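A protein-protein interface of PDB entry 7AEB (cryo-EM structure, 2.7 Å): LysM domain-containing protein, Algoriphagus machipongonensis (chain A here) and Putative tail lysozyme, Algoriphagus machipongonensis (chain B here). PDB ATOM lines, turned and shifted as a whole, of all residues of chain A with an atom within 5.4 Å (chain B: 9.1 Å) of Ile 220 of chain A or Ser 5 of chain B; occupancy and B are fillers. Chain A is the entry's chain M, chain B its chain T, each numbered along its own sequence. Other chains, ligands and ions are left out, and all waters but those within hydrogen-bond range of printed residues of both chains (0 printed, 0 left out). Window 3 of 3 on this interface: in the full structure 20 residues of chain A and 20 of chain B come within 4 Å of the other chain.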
ATOM      1  N   HIS A 174     -10.147 -27.872  12.196  1.00  0.00           N
ATOM      2  CA  HIS A 174      -9.681 -27.167  13.382  1.00  0.00           C
ATOM      3  C   HIS A 174      -9.579 -25.678  13.079  1.00  0.00           C
ATOM      4  O   HIS A 174      -9.363 -25.289  11.933  1.00  0.00           O
ATOM      5  CB  HIS A 174      -8.326 -27.725  13.827  1.00  0.00           C
ATOM      6  CG  HIS A 174      -7.834 -27.168  15.124  1.00  0.00           C
ATOM      7  ND1 HIS A 174      -8.563 -27.240  16.290  1.00  0.00           N
ATOM      8  CD2 HIS A 174      -6.688 -26.528  15.438  1.00  0.00           C
ATOM      9  CE1 HIS A 174      -7.887 -26.666  17.266  1.00  0.00           C
ATOM     10  NE2 HIS A 174      -6.745 -26.227  16.776  1.00  0.00           N
ATOM     11  N   TYR A 175      -9.758 -24.844  14.108  1.00  0.00           N
ATOM     12  CA  TYR A 175      -9.527 -23.408  13.989  1.00  0.00           C
ATOM     13  C   TYR A 175      -8.781 -22.893  15.216  1.00  0.00           C
ATOM     14  O   TYR A 175      -8.965 -23.390  16.327  1.00  0.00           O
ATOM     15  CB  TYR A 175     -10.848 -22.615  13.770  1.00  0.00           C
ATOM     16  CG  TYR A 175     -11.908 -22.734  14.849  1.00  0.00           C
ATOM     17  CD1 TYR A 175     -11.889 -21.908  15.970  1.00  0.00           C
ATOM     18  CD2 TYR A 175     -12.950 -23.637  14.729  1.00  0.00           C
ATOM     19  CE1 TYR A 175     -12.845 -22.012  16.950  1.00  0.00           C
ATOM     20  CE2 TYR A 175     -13.920 -23.744  15.707  1.00  0.00           C
ATOM     21  CZ  TYR A 175     -13.858 -22.931  16.814  1.00  0.00           C
ATOM     22  OH  TYR A 175     -14.819 -23.028  17.790  1.00  0.00           O
ATOM     23  N   VAL A 201      -1.361 -24.873   4.383  1.00  0.00           N
ATOM     24  CA  VAL A 201      -2.187 -24.120   5.318  1.00  0.00           C
ATOM     25  C   VAL A 201      -2.288 -22.667   4.876  1.00  0.00           C
ATOM     26  O   VAL A 201      -3.336 -22.026   5.024  1.00  0.00           O
ATOM     27  CB  VAL A 201      -1.619 -24.254   6.746  1.00  0.00           C
ATOM     28  CG1 VAL A 201      -2.452 -23.490   7.763  1.00  0.00           C
ATOM     29  CG2 VAL A 201      -1.534 -25.706   7.140  1.00  0.00           C
ATOM     30  N   ALA A 204      -4.737 -22.363   1.851  1.00  0.00           N
ATOM     31  CA  ALA A 204      -6.141 -22.551   2.182  1.00  0.00           C
ATOM     32  C   ALA A 204      -6.719 -21.355   2.918  1.00  0.00           C
ATOM     33  O   ALA A 204      -7.939 -21.259   3.075  1.00  0.00           O
ATOM     34  CB  ALA A 204      -6.317 -23.822   3.012  1.00  0.00           C
ATOM     35  N   ASN A 205      -5.873 -20.434   3.364  1.00  0.00           N
ATOM     36  CA  ASN A 205      -6.297 -19.242   4.077  1.00  0.00           C
ATOM     37  C   ASN A 205      -6.069 -17.965   3.283  1.00  0.00           C
ATOM     38  O   ASN A 205      -6.417 -16.883   3.761  1.00  0.00           O
ATOM     39  CB  ASN A 205      -5.570 -19.154   5.421  1.00  0.00           C
ATOM     40  CG  ASN A 205      -6.074 -20.167   6.420  1.00  0.00           C
ATOM     41  OD1 ASN A 205      -7.041 -19.923   7.129  1.00  0.00           O
ATOM     42  ND2 ASN A 205      -5.423 -21.314   6.478  1.00  0.00           N
ATOM     43  N   GLU A 218      -8.043 -15.375  12.505  1.00  0.00           N
ATOM     44  CA  GLU A 218      -8.520 -16.731  12.745  1.00  0.00           C
ATOM     45  C   GLU A 218      -8.252 -17.554  11.503  1.00  0.00           C
ATOM     46  O   GLU A 218      -8.686 -17.151  10.431  1.00  0.00           O
ATOM     47  CB  GLU A 218      -9.983 -16.777  13.205  1.00  0.00           C
ATOM     48  CG  GLU A 218     -10.246 -16.083  14.528  1.00  0.00           C
ATOM     49  CD  GLU A 218     -11.713 -15.998  14.916  1.00  0.00           C
ATOM     50  OE1 GLU A 218     -12.584 -16.322  14.077  1.00  0.00           O
ATOM     51  OE2 GLU A 218     -11.986 -15.662  16.090  1.00  0.00           O
ATOM     52  N   LEU A 219      -7.514 -18.662  11.653  1.00  0.00           N
ATOM     53  CA  LEU A 219      -7.120 -19.563  10.579  1.00  0.00           C
ATOM     54  C   LEU A 219      -7.912 -20.861  10.659  1.00  0.00           C
ATOM     55  O   LEU A 219      -8.426 -21.224  11.714  1.00  0.00           O
ATOM     56  CB  LEU A 219      -5.624 -19.884  10.648  1.00  0.00           C
ATOM     57  CG  LEU A 219      -4.611 -18.744  10.659  1.00  0.00           C
ATOM     58  CD1 LEU A 219      -3.276 -19.258  11.119  1.00  0.00           C
ATOM     59  CD2 LEU A 219      -4.484 -18.115   9.292  1.00  0.00           C
ATOM     60  N   ILE A 220      -8.017 -21.549   9.525  1.00  0.00           N
ATOM     61  CA  ILE A 220      -8.571 -22.895   9.458  1.00  0.00           C
ATOM     62  C   ILE A 220      -7.438 -23.873   9.196  1.00  0.00           C
ATOM     63  O   ILE A 220      -6.412 -23.519   8.609  1.00  0.00           O
ATOM     64  CB  ILE A 220      -9.662 -23.021   8.373  1.00  0.00           C
ATOM     65  CG1 ILE A 220      -9.115 -22.621   7.002  1.00  0.00           C
ATOM     66  CG2 ILE A 220     -10.873 -22.179   8.733  1.00  0.00           C
ATOM     67  CD1 ILE A 220      -9.977 -23.046   5.855  1.00  0.00           C
ATOM     68  N   PHE A 221      -7.610 -25.105   9.662  1.00  0.00           N
ATOM     69  CA  PHE A 221      -6.642 -26.172   9.425  1.00  0.00           C
ATOM     70  C   PHE A 221      -7.383 -27.373   8.849  1.00  0.00           C
ATOM     71  O   PHE A 221      -7.978 -28.151   9.609  1.00  0.00           O
ATOM     72  CB  PHE A 221      -5.906 -26.541  10.711  1.00  0.00           C
ATOM     73  CG  PHE A 221      -4.934 -25.494  11.177  1.00  0.00           C
ATOM     74  CD1 PHE A 221      -5.359 -24.432  11.957  1.00  0.00           C
ATOM     75  CD2 PHE A 221      -3.599 -25.563  10.825  1.00  0.00           C
ATOM     76  CE1 PHE A 221      -4.475 -23.462  12.373  1.00  0.00           C
ATOM     77  CE2 PHE A 221      -2.709 -24.597  11.249  1.00  0.00           C
ATOM     78  CZ  PHE A 221      -3.150 -23.545  12.021  1.00  0.00           C
ATOM     79  N   PRO A 222      -7.396 -27.546   7.527  1.00  0.00           N
ATOM     80  CA  PRO A 222      -8.154 -28.649   6.927  1.00  0.00           C
ATOM     81  C   PRO A 222      -7.511 -29.996   7.199  1.00  0.00           C
ATOM     82  O   PRO A 222      -6.295 -30.081   7.431  1.00  0.00           O
ATOM     83  CB  PRO A 222      -8.117 -28.314   5.426  1.00  0.00           C
ATOM     84  CG  PRO A 222      -7.932 -26.870   5.386  1.00  0.00           C
ATOM     85  CD  PRO A 222      -7.015 -26.555   6.514  1.00  0.00           C
ATOM     86  N   LYS B   4     -14.989 -16.706   9.421  1.00  0.00           N
ATOM     87  CA  LYS B   4     -15.587 -17.795   8.647  1.00  0.00           C
ATOM     88  C   LYS B   4     -14.846 -19.106   8.870  1.00  0.00           C
ATOM     89  O   LYS B   4     -14.884 -20.048   8.085  1.00  0.00           O
ATOM     90  CB  LYS B   4     -15.669 -17.394   7.166  1.00  0.00           C
ATOM     91  CG  LYS B   4     -16.293 -18.400   6.214  1.00  0.00           C
ATOM     92  CD  LYS B   4     -16.346 -17.953   4.837  1.00  0.00           C
ATOM     93  CE  LYS B   4     -14.969 -17.752   4.269  1.00  0.00           C
ATOM     94  NZ  LYS B   4     -15.021 -17.258   2.865  1.00  0.00           N
ATOM     95  N   SER B   5     -14.033 -19.080   9.929  1.00  0.00           N
ATOM     96  CA  SER B   5     -13.319 -20.248  10.445  1.00  0.00           C
ATOM     97  C   SER B   5     -14.249 -21.245  11.164  1.00  0.00           C
ATOM     98  O   SER B   5     -14.139 -22.459  10.994  1.00  0.00           O
ATOM     99  CB  SER B   5     -12.190 -19.814  11.383  1.00  0.00           C
ATOM    100  OG  SER B   5     -12.695 -19.073  12.479  1.00  0.00           O
ATOM    101  N   LYS B   6     -15.166 -20.697  11.967  1.00  0.00           N
ATOM    102  CA  LYS B   6     -16.132 -21.447  12.764  1.00  0.00           C
ATOM    103  C   LYS B   6     -17.415 -21.674  11.966  1.00  0.00           C
ATOM    104  O   LYS B   6     -18.478 -21.181  12.321  1.00  0.00           O
ATOM    105  CB  LYS B   6     -16.429 -20.711  14.065  1.00  0.00           C
ATOM    106  CG  LYS B   6     -15.216 -20.418  14.921  1.00  0.00           C
ATOM    107  CD  LYS B   6     -15.592 -19.655  16.182  1.00  0.00           C
ATOM    108  CE  LYS B   6     -14.367 -19.334  17.018  1.00  0.00           C
ATOM    109  NZ  LYS B   6     -14.714 -18.581  18.254  1.00  0.00           N
ATOM    110  N   ASP B   7     -17.302 -22.416  10.864  1.00  0.00           N
ATOM    111  CA  ASP B   7     -18.433 -22.748   9.993  1.00  0.00           C
ATOM    112  C   ASP B   7     -18.941 -24.166  10.217  1.00  0.00           C
ATOM    113  O   ASP B   7     -19.941 -24.546   9.600  1.00  0.00           O
ATOM    114  CB  ASP B   7     -17.967 -22.581   8.557  1.00  0.00           C
ATOM    115  CG  ASP B   7     -17.697 -21.176   8.220  1.00  0.00           C
ATOM    116  OD1 ASP B   7     -17.500 -20.960   7.031  1.00  0.00           O
ATOM    117  OD2 ASP B   7     -17.815 -20.303   9.122  1.00  0.00           O
ATOM    118  N   PHE B   8     -18.282 -24.967  11.068  1.00  0.00           N
ATOM    119  CA  PHE B   8     -18.780 -26.317  11.335  1.00  0.00           C
ATOM    120  C   PHE B   8     -19.706 -26.378  12.531  1.00  0.00           C
ATOM    121  O   PHE B   8     -20.157 -27.468  12.898  1.00  0.00           O
ATOM    122  CB  PHE B   8     -17.650 -27.374  11.476  1.00  0.00           C
ATOM    123  CG  PHE B   8     -16.659 -27.157  12.580  1.00  0.00           C
ATOM    124  CD1 PHE B   8     -16.928 -27.515  13.893  1.00  0.00           C
ATOM    125  CD2 PHE B   8     -15.397 -26.711  12.269  1.00  0.00           C
ATOM    126  CE1 PHE B   8     -15.992 -27.355  14.864  1.00  0.00           C
ATOM    127  CE2 PHE B   8     -14.457 -26.560  13.245  1.00  0.00           C
ATOM    128  CZ  PHE B   8     -14.756 -26.880  14.542  1.00  0.00           C
ATOM    129  N   LEU B   9     -19.991 -25.257  13.156  1.00  0.00           N
ATOM    130  CA  LEU B   9     -20.998 -25.270  14.191  1.00  0.00           C
ATOM    131  C   LEU B   9     -22.353 -25.118  13.537  1.00  0.00           C
ATOM    132  O   LEU B   9     -23.361 -25.612  14.051  1.00  0.00           O
ATOM    133  CB  LEU B   9     -20.716 -24.168  15.221  1.00  0.00           C
ATOM    134  CG  LEU B   9     -19.368 -24.207  15.968  1.00  0.00           C
ATOM    135  CD1 LEU B   9     -19.268 -23.022  16.906  1.00  0.00           C
ATOM    136  CD2 LEU B   9     -19.186 -25.512  16.737  1.00  0.00           C
ATOM    137  N   GLY B  10     -22.360 -24.479  12.370  1.00  0.00           N
ATOM    138  CA  GLY B  10     -23.531 -24.380  11.532  1.00  0.00           C
ATOM    139  C   GLY B  10     -24.491 -23.255  11.876  1.00  0.00           C
ATOM    140  O   GLY B  10     -24.287 -22.462  12.797  1.00  0.00           O
ATOM    141  N   ALA B 118     -13.371 -27.016  19.897  1.00  0.00           N
ATOM    142  CA  ALA B 118     -12.606 -26.363  18.834  1.00  0.00           C
ATOM    143  C   ALA B 118     -12.363 -27.240  17.608  1.00  0.00           C
ATOM    144  O   ALA B 118     -11.791 -26.764  16.626  1.00  0.00           O
ATOM    145  CB  ALA B 118     -11.251 -25.914  19.368  1.00  0.00           C
ATOM    146  N   ASN B 120     -14.014 -30.624  15.040  1.00  0.00           N
ATOM    147  CA  ASN B 120     -15.308 -31.121  14.598  1.00  0.00           C
ATOM    148  C   ASN B 120     -15.549 -32.600  14.914  1.00  0.00           C
ATOM    149  O   ASN B 120     -14.784 -33.472  14.494  1.00  0.00           O
ATOM    150  CB  ASN B 120     -15.482 -30.879  13.116  1.00  0.00           C
ATOM    151  CG  ASN B 120     -16.863 -31.108  12.732  1.00  0.00           C
ATOM    152  OD1 ASN B 120     -17.760 -30.905  13.545  1.00  0.00           O
ATOM    153  ND2 ASN B 120     -17.078 -31.573  11.535  1.00  0.00           N
ATOM    154  N   PHE B 129     -19.452 -30.601   5.797  1.00  0.00           N
ATOM    155  CA  PHE B 129     -18.463 -31.330   6.575  1.00  0.00           C
ATOM    156  C   PHE B 129     -18.779 -32.798   6.730  1.00  0.00           C
ATOM    157  O   PHE B 129     -17.900 -33.621   6.476  1.00  0.00           O
ATOM    158  CB  PHE B 129     -18.308 -30.730   7.957  1.00  0.00           C
ATOM    159  CG  PHE B 129     -17.846 -29.358   7.926  1.00  0.00           C
ATOM    160  CD1 PHE B 129     -18.749 -28.336   7.979  1.00  0.00           C
ATOM    161  CD2 PHE B 129     -16.507 -29.077   7.822  1.00  0.00           C
ATOM    162  CE1 PHE B 129     -18.332 -27.055   7.927  1.00  0.00           C
ATOM    163  CE2 PHE B 129     -16.084 -27.784   7.774  1.00  0.00           C
ATOM    164  CZ  PHE B 129     -17.000 -26.771   7.830  1.00  0.00           C
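ND1 of His 174 of chain A lies within hydrogen-bond range of O of Ala 118 of chain B. The side-chain carboxylate (OE1) of Glu 218 of chain A lies within hydrogen-bond range of the side-chain hydroxyl (OG) of Ser 5 of chain B, 3.2 Å away.
The backbone NH (N) of Phe 221 of chain A lies within hydrogen-bond range of the backbone carbonyl oxygen (O) of His 174 of chain A, 2.9 Å away. N of Ile 220 of chain A sits at hydrogen-bond distance from OD1 of Asn 205 of chain A, at 3.1 Å.
Ser 5 of chain B touches Tyr 175 of chain A. Lys 6 of chain B touches Tyr 175 of chain A. Phe 8 of chain B touches Tyr 175 of chain A (CZ to CE2, 3.4 Å). N of Tyr 175 of chain A touches O of Ala 118 of chain B, at 3.8 Å. CA of Ser 5 of chain B touches CG2 of Ile 220 of chain A, 3.6 Å away.
Of chain B, only Ser 5 (3.6 Å) comes within 4 Å of Ile 220 of chain A. Of the printed residues of chain A, Phe 8 of chain B touches Tyr 175. Printed residues of chain A within 4 Å of Lys 6 of chain B: Tyr 175 (3.1 Å). Printed residues of chain A within 4 Å of Ala 118 of chain B: His 174 (3.3 Å) and Tyr 175 (3.8 Å). Printed residues of chain B within 4 Å of Glu 218 of chain A: Ser 5. Pro 222 of chain A touches none of the printed residues of chain B. The nearest residue of chain A that does not touch Ser 5 of chain B is Leu 219 of chain A (4.03 Å).
Of the 10 printed residues of chain B, 4 touch a printed residue of chain A. Printed residues of chain B that touch a printed residue of chain A: Ser 5, Lys 6, Phe 8 and Ala 118. Of the 10 printed residues of chain A, 4 touch a printed residue of chain B. Hydrophobic or aromatic side chains of chain A within 4 Å of the printed part of chain B: His 174, Tyr 175 and Ile 220. Among the printed residues, no Asp or Glu carboxylate lies within 4 Å of a Lys or Arg side-chain nitrogen of the other chain.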
